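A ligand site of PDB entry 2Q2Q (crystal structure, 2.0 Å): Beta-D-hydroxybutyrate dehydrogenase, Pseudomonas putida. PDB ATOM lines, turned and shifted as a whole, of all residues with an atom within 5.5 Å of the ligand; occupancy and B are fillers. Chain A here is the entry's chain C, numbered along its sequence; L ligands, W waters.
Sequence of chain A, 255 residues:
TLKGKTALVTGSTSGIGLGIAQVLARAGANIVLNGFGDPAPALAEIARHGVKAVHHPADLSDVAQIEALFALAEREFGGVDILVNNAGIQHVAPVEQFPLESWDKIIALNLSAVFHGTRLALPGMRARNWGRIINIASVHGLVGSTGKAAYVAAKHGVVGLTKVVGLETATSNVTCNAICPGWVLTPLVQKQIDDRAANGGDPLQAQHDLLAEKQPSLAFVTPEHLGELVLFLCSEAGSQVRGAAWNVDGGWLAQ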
ATOM      1  N   THR A  10       2.584  -7.325  19.816  1.00  0.00           N
ATOM      2  CA  THR A  10       2.391  -6.969  21.235  1.00  0.00           C
ATOM      3  C   THR A  10       2.851  -5.520  21.476  1.00  0.00           C
ATOM      4  O   THR A  10       3.607  -4.943  20.651  1.00  0.00           O
ATOM      5  CB  THR A  10       3.004  -7.959  22.249  1.00  0.00           C
ATOM      6  OG1 THR A  10       4.429  -8.066  22.047  1.00  0.00           O
ATOM      7  CG2 THR A  10       2.373  -9.347  22.056  1.00  0.00           C
ATOM      8  N   GLY A  11       2.348  -4.905  22.552  1.00  0.00           N
ATOM      9  CA  GLY A  11       2.743  -3.567  22.910  1.00  0.00           C
ATOM     10  C   GLY A  11       2.702  -2.633  21.715  1.00  0.00           C
ATOM     11  O   GLY A  11       3.665  -1.953  21.415  1.00  0.00           O
ATOM     12  N   SER A  12       1.569  -2.625  21.024  1.00  0.00           N
ATOM     13  CA  SER A  12       1.411  -1.861  19.801  1.00  0.00           C
ATOM     14  C   SER A  12       0.371  -0.769  19.885  1.00  0.00           C
ATOM     15  O   SER A  12      -0.055  -0.204  18.845  1.00  0.00           O
ATOM     16  CB  SER A  12       1.103  -2.792  18.631  1.00  0.00           C
ATOM     17  OG  SER A  12      -0.057  -3.534  18.916  1.00  0.00           O
ATOM     18  N   THR A  13      -0.052  -0.431  21.105  1.00  0.00           N
ATOM     19  CA  THR A  13      -0.898   0.770  21.263  1.00  0.00           C
ATOM     20  C   THR A  13      -0.079   2.032  21.007  1.00  0.00           C
ATOM     21  O   THR A  13      -0.622   3.019  20.489  1.00  0.00           O
ATOM     22  CB  THR A  13      -1.805   0.805  22.574  1.00  0.00           C
ATOM     23  OG1 THR A  13      -1.020   0.600  23.787  1.00  0.00           O
ATOM     24  CG2 THR A  13      -2.938  -0.245  22.473  1.00  0.00           C
ATOM     25  N   SER A  14       1.246   1.928  21.258  1.00  0.00           N
ATOM     26  CA  SER A  14       2.224   3.053  21.253  1.00  0.00           C
ATOM     27  C   SER A  14       3.644   2.681  20.778  1.00  0.00           C
ATOM     28  O   SER A  14       4.107   1.552  21.019  1.00  0.00           O
ATOM     29  CB  SER A  14       2.353   3.681  22.652  1.00  0.00           C
ATOM     30  OG  SER A  14       1.573   4.864  22.781  1.00  0.00           O
ATOM     31  N   GLY A  15       4.324   3.642  20.123  1.00  0.00           N
ATOM     32  CA  GLY A  15       5.783   3.602  19.936  1.00  0.00           C
ATOM     33  C   GLY A  15       6.329   2.603  18.911  1.00  0.00           C
ATOM     34  O   GLY A  15       5.890   2.594  17.730  1.00  0.00           O
ATOM     35  N   ILE A  16       7.303   1.795  19.345  1.00  0.00           N
ATOM     36  CA  ILE A  16       7.960   0.858  18.435  1.00  0.00           C
ATOM     37  C   ILE A  16       6.877  -0.074  17.947  1.00  0.00           C
ATOM     38  O   ILE A  16       6.611  -0.130  16.737  1.00  0.00           O
ATOM     39  CB  ILE A  16       9.165   0.148  19.115  1.00  0.00           C
ATOM     40  CG1 ILE A  16      10.379   1.100  19.102  1.00  0.00           C
ATOM     41  CG2 ILE A  16       9.509  -1.169  18.414  1.00  0.00           C
ATOM     42  CD1 ILE A  16      11.459   0.709  19.975  1.00  0.00           C
ATOM     43  N   GLY A  17       6.187  -0.713  18.901  1.00  0.00           N
ATOM     44  CA  GLY A  17       4.933  -1.465  18.629  1.00  0.00           C
ATOM     45  C   GLY A  17       4.043  -0.889  17.534  1.00  0.00           C
ATOM     46  O   GLY A  17       3.820  -1.538  16.483  1.00  0.00           O
ATOM     47  N   ASN A  34      -2.232  -4.730  20.536  1.00  0.00           N
ATOM     48  CA  ASN A  34      -2.154  -5.008  21.975  1.00  0.00           C
ATOM     49  C   ASN A  34      -1.689  -3.791  22.764  1.00  0.00           C
ATOM     50  O   ASN A  34      -0.915  -2.950  22.246  1.00  0.00           O
ATOM     51  CB  ASN A  34      -1.198  -6.173  22.275  1.00  0.00           C
ATOM     52  CG  ASN A  34      -1.079  -6.442  23.748  1.00  0.00           C
ATOM     53  OD1 ASN A  34      -2.086  -6.651  24.419  1.00  0.00           O
ATOM     54  ND2 ASN A  34       0.125  -6.417  24.269  1.00  0.00           N
ATOM     55  N   GLY A  35      -2.160  -3.696  24.006  1.00  0.00           N
ATOM     56  CA  GLY A  35      -1.522  -2.869  25.013  1.00  0.00           C
ATOM     57  C   GLY A  35      -2.456  -1.968  25.799  1.00  0.00           C
ATOM     58  O   GLY A  35      -3.668  -1.971  25.561  1.00  0.00           O
ATOM     59  N   PHE A  36      -1.870  -1.190  26.700  1.00  0.00           N
ATOM     60  CA  PHE A  36      -2.594  -0.278  27.604  1.00  0.00           C
ATOM     61  C   PHE A  36      -2.801   1.078  26.982  1.00  0.00           C
ATOM     62  O   PHE A  36      -2.220   1.405  25.948  1.00  0.00           O
ATOM     63  CB  PHE A  36      -1.816  -0.092  28.913  1.00  0.00           C
ATOM     64  CG  PHE A  36      -1.388  -1.378  29.557  1.00  0.00           C
ATOM     65  CD1 PHE A  36      -2.143  -2.564  29.388  1.00  0.00           C
ATOM     66  CD2 PHE A  36      -0.252  -1.422  30.371  1.00  0.00           C
ATOM     67  CE1 PHE A  36      -1.770  -3.755  29.972  1.00  0.00           C
ATOM     68  CE2 PHE A  36       0.139  -2.612  30.982  1.00  0.00           C
ATOM     69  CZ  PHE A  36      -0.628  -3.788  30.781  1.00  0.00           C
ATOM     70  N   GLY A  37      -3.659   1.879  27.624  1.00  0.00           N
ATOM     71  CA  GLY A  37      -3.701   3.287  27.352  1.00  0.00           C
ATOM     72  C   GLY A  37      -4.775   3.815  26.438  1.00  0.00           C
ATOM     73  O   GLY A  37      -4.997   5.037  26.461  1.00  0.00           O
ATOM     74  N   ALA A  58      -4.780  -7.100  26.665  1.00  0.00           N
ATOM     75  CA  ALA A  58      -4.096  -8.000  27.600  1.00  0.00           C
ATOM     76  C   ALA A  58      -2.810  -7.413  28.249  1.00  0.00           C
ATOM     77  O   ALA A  58      -1.959  -6.807  27.584  1.00  0.00           O
ATOM     78  CB  ALA A  58      -3.789  -9.360  26.951  1.00  0.00           C
ATOM     79  N   ASP A  59      -2.737  -7.604  29.574  1.00  0.00           N
ATOM     80  CA  ASP A  59      -1.531  -7.487  30.390  1.00  0.00           C
ATOM     81  C   ASP A  59      -0.825  -8.847  30.240  1.00  0.00           C
ATOM     82  O   ASP A  59      -1.250  -9.873  30.797  1.00  0.00           O
ATOM     83  CB  ASP A  59      -1.966  -7.217  31.844  1.00  0.00           C
ATOM     84  CG  ASP A  59      -0.833  -7.307  32.853  1.00  0.00           C
ATOM     85  OD1 ASP A  59       0.224  -7.961  32.624  1.00  0.00           O
ATOM     86  OD2 ASP A  59      -1.023  -6.729  33.937  1.00  0.00           O
ATOM     87  N   LEU A  60       0.252  -8.832  29.464  1.00  0.00           N
ATOM     88  CA  LEU A  60       1.008 -10.038  29.168  1.00  0.00           C
ATOM     89  C   LEU A  60       1.899 -10.572  30.261  1.00  0.00           C
ATOM     90  O   LEU A  60       2.543 -11.591  30.035  1.00  0.00           O
ATOM     91  CB  LEU A  60       1.861  -9.879  27.884  1.00  0.00           C
ATOM     92  CG  LEU A  60       1.067  -9.374  26.681  1.00  0.00           C
ATOM     93  CD1 LEU A  60       2.012  -9.066  25.542  1.00  0.00           C
ATOM     94  CD2 LEU A  60      -0.085 -10.344  26.271  1.00  0.00           C
ATOM     95  N   SER A  61       1.953  -9.912  31.426  1.00  0.00           N
ATOM     96  CA  SER A  61       2.594 -10.528  32.586  1.00  0.00           C
ATOM     97  C   SER A  61       1.661 -11.612  33.156  1.00  0.00           C
ATOM     98  O   SER A  61       2.072 -12.308  34.076  1.00  0.00           O
ATOM     99  CB  SER A  61       2.973  -9.497  33.680  1.00  0.00           C
ATOM    100  OG  SER A  61       1.876  -9.130  34.513  1.00  0.00           O
ATOM    101  N   ASN A  86       6.866  -7.794  21.165  1.00  0.00           N
ATOM    102  CA  ASN A  86       7.417  -6.463  21.322  1.00  0.00           C
ATOM    103  C   ASN A  86       7.193  -5.855  22.709  1.00  0.00           C
ATOM    104  O   ASN A  86       8.102  -5.194  23.243  1.00  0.00           O
ATOM    105  CB  ASN A  86       6.839  -5.537  20.269  1.00  0.00           C
ATOM    106  CG  ASN A  86       7.194  -4.059  20.510  1.00  0.00           C
ATOM    107  OD1 ASN A  86       8.230  -3.583  20.028  1.00  0.00           O
ATOM    108  ND2 ASN A  86       6.300  -3.320  21.161  1.00  0.00           N
ATOM    109  N   ALA A  87       6.018  -6.059  23.299  1.00  0.00           N
ATOM    110  CA  ALA A  87       5.742  -5.505  24.632  1.00  0.00           C
ATOM    111  C   ALA A  87       6.953  -5.543  25.624  1.00  0.00           C
ATOM    112  O   ALA A  87       7.612  -6.592  25.818  1.00  0.00           O
ATOM    113  CB  ALA A  87       4.502  -6.180  25.245  1.00  0.00           C
ATOM    114  N   GLY A  88       7.250  -4.415  26.259  1.00  0.00           N
ATOM    115  CA  GLY A  88       8.414  -4.370  27.155  1.00  0.00           C
ATOM    116  C   GLY A  88       8.362  -3.207  28.092  1.00  0.00           C
ATOM    117  O   GLY A  88       7.846  -2.136  27.744  1.00  0.00           O
ATOM    118  N   ILE A  89       8.841  -3.433  29.316  1.00  0.00           N
ATOM    119  CA  ILE A  89       9.011  -2.357  30.279  1.00  0.00           C
ATOM    120  C   ILE A  89      10.501  -2.169  30.663  1.00  0.00           C
ATOM    121  O   ILE A  89      11.387  -2.737  30.005  1.00  0.00           O
ATOM    122  CB  ILE A  89       8.127  -2.562  31.515  1.00  0.00           C
ATOM    123  CG1 ILE A  89       8.487  -3.877  32.241  1.00  0.00           C
ATOM    124  CG2 ILE A  89       6.638  -2.475  31.117  1.00  0.00           C
ATOM    125  CD1 ILE A  89       7.655  -4.188  33.469  1.00  0.00           C
ATOM    126  N   LYS A 105       8.134  -9.000  37.400  1.00  0.00           N
ATOM    127  CA  LYS A 105       7.370  -8.308  36.301  1.00  0.00           C
ATOM    128  C   LYS A 105       8.157  -8.202  34.966  1.00  0.00           C
ATOM    129  O   LYS A 105       7.646  -8.581  33.929  1.00  0.00           O
ATOM    130  CB  LYS A 105       6.832  -6.915  36.722  1.00  0.00           C
ATOM    131  CG  LYS A 105       5.913  -6.217  35.645  1.00  0.00           C
ATOM    132  CD  LYS A 105       4.347  -6.198  35.936  1.00  0.00           C
ATOM    133  CE  LYS A 105       3.494  -5.626  34.701  1.00  0.00           C
ATOM    134  NZ  LYS A 105       1.959  -5.562  34.897  1.00  0.00           N
ATOM    135  N   LEU A 109       6.945 -10.138  31.566  1.00  0.00           N
ATOM    136  CA  LEU A 109       6.622  -9.390  30.337  1.00  0.00           C
ATOM    137  C   LEU A 109       7.677  -9.571  29.305  1.00  0.00           C
ATOM    138  O   LEU A 109       7.388 -10.053  28.201  1.00  0.00           O
ATOM    139  CB  LEU A 109       6.482  -7.877  30.557  1.00  0.00           C
ATOM    140  CG  LEU A 109       5.473  -7.031  29.714  1.00  0.00           C
ATOM    141  CD1 LEU A 109       5.982  -5.589  29.538  1.00  0.00           C
ATOM    142  CD2 LEU A 109       5.099  -7.586  28.383  1.00  0.00           C
ATOM    143  N   ASN A 110       8.912  -9.184  29.648  1.00  0.00           N
ATOM    144  CA  ASN A 110       9.980  -9.094  28.688  1.00  0.00           C
ATOM    145  C   ASN A 110      10.486 -10.487  28.241  1.00  0.00           C
ATOM    146  O   ASN A 110      11.064 -10.637  27.161  1.00  0.00           O
ATOM    147  CB  ASN A 110      11.134  -8.235  29.190  1.00  0.00           C
ATOM    148  CG  ASN A 110      10.730  -6.831  29.538  1.00  0.00           C
ATOM    149  OD1 ASN A 110      11.568  -5.911  29.557  1.00  0.00           O
ATOM    150  ND2 ASN A 110       9.469  -6.624  29.816  1.00  0.00           N
ATOM    151  N   ILE A 136      11.401  -8.302  19.307  1.00  0.00           N
ATOM    152  CA  ILE A 136      12.096  -7.063  19.597  1.00  0.00           C
ATOM    153  C   ILE A 136      12.791  -7.252  20.923  1.00  0.00           C
ATOM    154  O   ILE A 136      12.119  -7.204  22.021  1.00  0.00           O
ATOM    155  CB  ILE A 136      11.125  -5.936  19.756  1.00  0.00           C
ATOM    156  CG1 ILE A 136      10.244  -5.881  18.511  1.00  0.00           C
ATOM    157  CG2 ILE A 136      11.951  -4.649  19.991  1.00  0.00           C
ATOM    158  CD1 ILE A 136      11.057  -5.829  17.067  1.00  0.00           C
ATOM    159  N   ALA A 137      14.087  -7.601  20.836  1.00  0.00           N
ATOM    160  CA  ALA A 137      14.919  -7.722  22.001  1.00  0.00           C
ATOM    161  C   ALA A 137      15.566  -6.359  22.163  1.00  0.00           C
ATOM    162  O   ALA A 137      14.867  -5.339  22.150  1.00  0.00           O
ATOM    163  CB  ALA A 137      15.960  -8.926  21.906  1.00  0.00           C
ATOM    164  N   SER A 138      16.864  -6.281  22.226  1.00  0.00           N
ATOM    165  CA  SER A 138      17.510  -4.972  22.505  1.00  0.00           C
ATOM    166  C   SER A 138      18.998  -5.204  22.324  1.00  0.00           C
ATOM    167  O   SER A 138      19.407  -6.347  22.337  1.00  0.00           O
ATOM    168  CB  SER A 138      17.228  -4.475  23.963  1.00  0.00           C
ATOM    169  OG  SER A 138      18.245  -3.550  24.384  1.00  0.00           O
ATOM    170  N   VAL A 139      19.787  -4.161  22.111  1.00  0.00           N
ATOM    171  CA  VAL A 139      21.224  -4.241  22.391  1.00  0.00           C
ATOM    172  C   VAL A 139      21.553  -5.005  23.711  1.00  0.00           C
ATOM    173  O   VAL A 139      22.596  -5.763  23.809  1.00  0.00           O
ATOM    174  CB  VAL A 139      21.932  -2.851  22.374  1.00  0.00           C
ATOM    175  CG1 VAL A 139      22.026  -2.270  20.959  1.00  0.00           C
ATOM    176  CG2 VAL A 139      21.293  -1.838  23.342  1.00  0.00           C
ATOM    177  N   TYR A 151      16.240  -6.396  33.015  1.00  0.00           N
ATOM    178  CA  TYR A 151      16.089  -6.125  31.621  1.00  0.00           C
ATOM    179  C   TYR A 151      17.120  -6.858  30.768  1.00  0.00           C
ATOM    180  O   TYR A 151      16.757  -7.492  29.740  1.00  0.00           O
ATOM    181  CB  TYR A 151      16.242  -4.612  31.438  1.00  0.00           C
ATOM    182  CG  TYR A 151      15.804  -4.109  30.076  1.00  0.00           C
ATOM    183  CD1 TYR A 151      16.728  -3.975  29.037  1.00  0.00           C
ATOM    184  CD2 TYR A 151      14.448  -3.796  29.796  1.00  0.00           C
ATOM    185  CE1 TYR A 151      16.361  -3.497  27.777  1.00  0.00           C
ATOM    186  CE2 TYR A 151      14.051  -3.332  28.484  1.00  0.00           C
ATOM    187  CZ  TYR A 151      15.035  -3.169  27.512  1.00  0.00           C
ATOM    188  OH  TYR A 151      14.743  -2.711  26.229  1.00  0.00           O
ATOM    189  N   LYS A 155      16.191  -9.805  28.077  1.00  0.00           N
ATOM    190  CA  LYS A 155      16.517  -9.692  26.663  1.00  0.00           C
ATOM    191  C   LYS A 155      17.628 -10.687  26.190  1.00  0.00           C
ATOM    192  O   LYS A 155      17.555 -11.156  25.091  1.00  0.00           O
ATOM    193  CB  LYS A 155      16.889  -8.251  26.273  1.00  0.00           C
ATOM    194  CG  LYS A 155      15.719  -7.257  26.478  1.00  0.00           C
ATOM    195  CD  LYS A 155      14.559  -7.497  25.463  1.00  0.00           C
ATOM    196  CE  LYS A 155      13.436  -6.550  25.707  1.00  0.00           C
ATOM    197  NZ  LYS A 155      12.568  -6.225  24.534  1.00  0.00           N
ATOM    198  N   CYS A 180      17.476  -6.315  17.568  1.00  0.00           N
ATOM    199  CA  CYS A 180      18.101  -5.770  18.759  1.00  0.00           C
ATOM    200  C   CYS A 180      18.387  -4.264  18.601  1.00  0.00           C
ATOM    201  O   CYS A 180      19.465  -3.892  18.141  1.00  0.00           O
ATOM    202  CB  CYS A 180      19.393  -6.532  19.054  1.00  0.00           C
ATOM    203  SG  CYS A 180      19.237  -8.293  19.334  1.00  0.00           S
ATOM    204  N   PRO A 181      17.392  -3.395  18.865  1.00  0.00           N
ATOM    205  CA  PRO A 181      17.699  -1.963  18.630  1.00  0.00           C
ATOM    206  C   PRO A 181      18.548  -1.297  19.702  1.00  0.00           C
ATOM    207  O   PRO A 181      18.505  -1.757  20.834  1.00  0.00           O
ATOM    208  CB  PRO A 181      16.300  -1.277  18.556  1.00  0.00           C
ATOM    209  CG  PRO A 181      15.286  -2.367  19.060  1.00  0.00           C
ATOM    210  CD  PRO A 181      15.962  -3.667  19.184  1.00  0.00           C
ATOM    211  N   GLY A 182      19.298  -0.247  19.369  1.00  0.00           N
ATOM    212  CA  GLY A 182      19.772   0.658  20.405  1.00  0.00           C
ATOM    213  C   GLY A 182      18.669   1.673  20.771  1.00  0.00           C
ATOM    214  O   GLY A 182      17.437   1.391  20.676  1.00  0.00           O
ATOM    215  N   TRP A 183      19.104   2.850  21.202  1.00  0.00           N
ATOM    216  CA  TRP A 183      18.175   3.884  21.634  1.00  0.00           C
ATOM    217  C   TRP A 183      17.192   4.279  20.541  1.00  0.00           C
ATOM    218  O   TRP A 183      17.572   4.700  19.420  1.00  0.00           O
ATOM    219  CB  TRP A 183      18.914   5.166  22.019  1.00  0.00           C
ATOM    220  CG  TRP A 183      19.869   5.132  23.172  1.00  0.00           C
ATOM    221  CD1 TRP A 183      21.212   5.530  23.162  1.00  0.00           C
ATOM    222  CD2 TRP A 183      19.581   4.763  24.520  1.00  0.00           C
ATOM    223  NE1 TRP A 183      21.750   5.415  24.419  1.00  0.00           N
ATOM    224  CE2 TRP A 183      20.779   4.943  25.266  1.00  0.00           C
ATOM    225  CE3 TRP A 183      18.441   4.310  25.172  1.00  0.00           C
ATOM    226  CZ2 TRP A 183      20.860   4.647  26.625  1.00  0.00           C
ATOM    227  CZ3 TRP A 183      18.506   4.018  26.519  1.00  0.00           C
ATOM    228  CH2 TRP A 183      19.714   4.196  27.234  1.00  0.00           C
ATOM    229  N   VAL A 184      15.908   4.176  20.885  1.00  0.00           N
ATOM    230  CA  VAL A 184      14.842   4.759  20.067  1.00  0.00           C
ATOM    231  C   VAL A 184      14.218   5.919  20.846  1.00  0.00           C
ATOM    232  O   VAL A 184      14.020   5.814  22.053  1.00  0.00           O
ATOM    233  CB  VAL A 184      13.759   3.722  19.762  1.00  0.00           C
ATOM    234  CG1 VAL A 184      12.714   4.300  18.882  1.00  0.00           C
ATOM    235  CG2 VAL A 184      14.414   2.446  19.123  1.00  0.00           C
ATOM    236  N   LEU A 185      13.909   7.035  20.180  1.00  0.00           N
ATOM    237  CA  LEU A 185      13.332   8.172  20.953  1.00  0.00           C
ATOM    238  C   LEU A 185      11.837   7.893  21.168  1.00  0.00           C
ATOM    239  O   LEU A 185      11.063   7.894  20.190  1.00  0.00           O
ATOM    240  CB  LEU A 185      13.604   9.534  20.286  1.00  0.00           C
ATOM    241  CG  LEU A 185      13.250  10.816  21.074  1.00  0.00           C
ATOM    242  CD1 LEU A 185      13.551  10.713  22.573  1.00  0.00           C
ATOM    243  CD2 LEU A 185      13.901  12.073  20.489  1.00  0.00           C
ATOM    244  N   THR A 186      11.479   7.527  22.421  1.00  0.00           N
ATOM    245  CA  THR A 186      10.129   7.102  22.849  1.00  0.00           C
ATOM    246  C   THR A 186       9.928   7.531  24.343  1.00  0.00           C
ATOM    247  O   THR A 186      10.896   7.563  25.119  1.00  0.00           O
ATOM    248  CB  THR A 186       9.848   5.530  22.696  1.00  0.00           C
ATOM    249  OG1 THR A 186      10.502   4.790  23.735  1.00  0.00           O
ATOM    250  CG2 THR A 186      10.243   4.931  21.304  1.00  0.00           C
ATOM    251  N   PRO A 187       8.692   7.872  24.762  1.00  0.00           N
ATOM    252  CA  PRO A 187       8.448   8.133  26.196  1.00  0.00           C
ATOM    253  C   PRO A 187       9.321   7.318  27.185  1.00  0.00           C
ATOM    254  O   PRO A 187       9.830   7.883  28.159  1.00  0.00           O
ATOM    255  CB  PRO A 187       6.984   7.752  26.361  1.00  0.00           C
ATOM    256  CG  PRO A 187       6.375   8.036  25.008  1.00  0.00           C
ATOM    257  CD  PRO A 187       7.465   8.052  23.971  1.00  0.00           C
ATOM    258  N   LEU A 188       9.499   6.011  26.926  1.00  0.00           N
ATOM    259  CA  LEU A 188      10.245   5.060  27.808  1.00  0.00           C
ATOM    260  C   LEU A 188      11.784   5.226  27.680  1.00  0.00           C
ATOM    261  O   LEU A 188      12.565   4.708  28.494  1.00  0.00           O
ATOM    262  CB  LEU A 188       9.769   3.601  27.565  1.00  0.00           C
ATOM    263  CG  LEU A 188      10.110   2.390  28.482  1.00  0.00           C
ATOM    264  CD1 LEU A 188       8.832   1.670  29.042  1.00  0.00           C
ATOM    265  CD2 LEU A 188      11.044   1.392  27.778  1.00  0.00           C
ATOM    266  N   VAL A 189      12.210   5.959  26.655  1.00  0.00           N
ATOM    267  CA  VAL A 189      13.548   6.504  26.570  1.00  0.00           C
ATOM    268  C   VAL A 189      13.617   7.957  27.124  1.00  0.00           C
ATOM    269  O   VAL A 189      14.463   8.238  27.976  1.00  0.00           O
ATOM    270  CB  VAL A 189      14.106   6.429  25.129  1.00  0.00           C
ATOM    271  CG1 VAL A 189      14.782   7.741  24.706  1.00  0.00           C
ATOM    272  CG2 VAL A 189      15.071   5.203  24.955  1.00  0.00           C
HETATM  273  P1  LIG L   1       6.914   2.159  24.892  1.00  0.00           P
HETATM  274  O1  LIG L   1       6.775   2.186  26.383  1.00  0.00           O
HETATM  275  O2  LIG L   1       6.892   3.438  24.088  1.00  0.00           O
HETATM  276  O3  LIG L   1       5.819   1.065  24.318  1.00  0.00           O
HETATM  277  C1  LIG L   1       5.565  -0.152  25.020  1.00  0.00           C
HETATM  278  C2  LIG L   1       4.213  -0.770  24.675  1.00  0.00           C
HETATM  279  O4  LIG L   1       4.036  -2.002  25.370  1.00  0.00           O
HETATM  280  C3  LIG L   1       3.013   0.136  25.044  1.00  0.00           C
HETATM  281  O5  LIG L   1       2.000   0.085  24.058  1.00  0.00           O
HETATM  282  C4  LIG L   1       2.460  -0.511  26.312  1.00  0.00           C
HETATM  283  O6  LIG L   1       1.081  -0.232  26.590  1.00  0.00           O
HETATM  284  C5  LIG L   1       2.758  -1.988  26.031  1.00  0.00           C
HETATM  285  N1  LIG L   1       2.819  -2.678  27.311  1.00  0.00           N
HETATM  286  C6  LIG L   1       3.489  -2.223  28.440  1.00  0.00           C
HETATM  287  N2  LIG L   1       3.324  -3.126  29.440  1.00  0.00           N
HETATM  288  C7  LIG L   1       2.536  -4.129  28.936  1.00  0.00           C
HETATM  289  C8  LIG L   1       2.077  -5.258  29.534  1.00  0.00           C
HETATM  290  N3  LIG L   1       2.191  -5.307  30.859  1.00  0.00           N
HETATM  291  N4  LIG L   1       1.321  -6.151  28.821  1.00  0.00           N
HETATM  292  C9  LIG L   1       0.975  -5.868  27.508  1.00  0.00           C
HETATM  293  N5  LIG L   1       1.406  -4.705  26.908  1.00  0.00           N
HETATM  294  C10 LIG L   1       2.202  -3.866  27.615  1.00  0.00           C
HETATM  295  O7  LIG L   1       8.421   1.531  24.701  1.00  0.00           O
HETATM  296  P2  LIG L   1       9.069   1.166  23.264  1.00  0.00           P
HETATM  297  O8  LIG L   1      10.305   2.008  23.193  1.00  0.00           O
HETATM  298  O9  LIG L   1       8.041   1.496  22.225  1.00  0.00           O
HETATM  299  O10 LIG L   1       9.259  -0.426  23.625  1.00  0.00           O
HETATM  300  C11 LIG L   1       8.897  -1.497  22.770  1.00  0.00           C
HETATM  301  C12 LIG L   1       9.917  -2.650  22.760  1.00  0.00           C
HETATM  302  O11 LIG L   1      11.076  -2.214  22.093  1.00  0.00           O
HETATM  303  C13 LIG L   1      10.360  -3.132  24.157  1.00  0.00           C
HETATM  304  O12 LIG L   1      10.370  -4.536  24.352  1.00  0.00           O
HETATM  305  C14 LIG L   1      11.771  -2.572  24.328  1.00  0.00           C
HETATM  306  O13 LIG L   1      12.517  -3.370  25.219  1.00  0.00           O
HETATM  307  C15 LIG L   1      12.216  -2.574  22.879  1.00  0.00           C
HETATM  308  N6  LIG L   1      13.408  -1.718  22.735  1.00  0.00           N
HETATM  309  C16 LIG L   1      13.262  -0.351  22.852  1.00  0.00           C
HETATM  310  C17 LIG L   1      14.369   0.494  22.769  1.00  0.00           C
HETATM  311  C18 LIG L   1      14.163   1.906  23.212  1.00  0.00           C
HETATM  312  O14 LIG L   1      15.300   2.766  23.286  1.00  0.00           O
HETATM  313  N7  LIG L   1      12.889   2.267  23.501  1.00  0.00           N
HETATM  314  C19 LIG L   1      15.649  -0.061  22.570  1.00  0.00           C
HETATM  315  C20 LIG L   1      15.800  -1.459  22.450  1.00  0.00           C
HETATM  316  C21 LIG L   1      14.665  -2.280  22.530  1.00  0.00           C
HETATM  317  O   HOH W   1      17.694  -0.437  25.108  1.00  0.00           O
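Gly 11 touches the ligand (CA to O4, 3.2 Å). Gly 15 touches the ligand. Gly 35 touches the ligand (CA to N5, 3.9 Å). O of Ala 58 touches C9 of the ligand, 3.1 Å away. Asp 59 touches the ligand. O of Ala 87 touches O12 of the ligand, at 3.7 Å. CA of Gly 88 touches O12 of the ligand, 3.4 Å away. Ile 89 touches the ligand (CG2 to N2, 3.8 Å). Leu 109 touches the ligand (CD1 to N2, 3.6 Å). Ile 136 touches the ligand. Ala 137 touches the ligand. CB of Ser 138 touches C20 of the ligand, at 3.7 Å. Pro 181 touches the ligand. Gly 182 touches the ligand (O to C19, 3.0 Å). CA of Trp 183 touches O14 of the ligand (3.5 Å). Leu 188 touches the ligand (CD1 to O1, 3.4 Å). CG2 of Val 189 touches O14 of the ligand, at 3.0 Å. Hydrophobic or aromatic side chains that line the ligand: Ile 16, Phe 36, Leu 60, Ala 87, Ile 89, Leu 109, Ile 136, Tyr 151, Pro 181, Trp 183, Val 184, Leu 188 and Val 189. The nearest printed residue that does not touch the ligand is Lys 105 (4.1 Å).
An oxygen (O8) of the ligand sits at hydrogen-bond distance from the side-chain hydroxyl of Thr 186 (2.8 Å). The backbone NH (N) of Leu 60 is in hydrogen-bond range of a nitrogen (N4) of the ligand (3.0 Å). O5 of the ligand lies within hydrogen-bond range of OG1 of Thr 13 (3.1 Å). An oxygen (O14) of the ligand lies within hydrogen-bond range of the backbone NH (N) of Val 184 (2.9 Å). N of Ser 14 sits at hydrogen-bond distance from O5 of the ligand, 3.4 Å away. The side-chain amino group (NZ) of Lys 155 is in hydrogen-bond range of an oxygen (O12) of the ligand, at 2.8 Å. OH of Tyr 151 sits at hydrogen-bond distance from O13 of the ligand (2.5 Å). O9 of the ligand is in hydrogen-bond range of N of Ile 16, at 3.0 Å. The backbone NH (N) of Phe 36 is in hydrogen-bond range of an oxygen (O6) of the ligand. The backbone carbonyl oxygen (O) of Asn 86 lies within hydrogen-bond range of an oxygen (O12) of the ligand (2.6 Å). N5 of the ligand lies close to ND2 of Asn 34.
OD1 of Asn 34 lies close to O of Ala 58, 3.2 Å away. ND2 of Asn 86 is in hydrogen-bond range of O of Gly 11 (3.0 Å). The side-chain hydroxyl (OG1) of Thr 13 lies within hydrogen-bond range of the backbone carbonyl oxygen (O) of Phe 36, 2.6 Å away. The side-chain carboxylate (OD1) of Asp 59 sits at hydrogen-bond distance from the side-chain hydroxyl (OG) of Ser 61, 2.8 Å away. The backbone carbonyl oxygen (O) of Ser 138 sits close to the side-chain sulfur (SG) of Cys 180. OG1 of Thr 10 lies within hydrogen-bond range of N of Asn 86. O of Asn 34 is in hydrogen-bond range of N of Thr 13, at 2.9 Å. O of Asn 34 sits at hydrogen-bond distance from N of Ser 12, at 2.8 Å.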
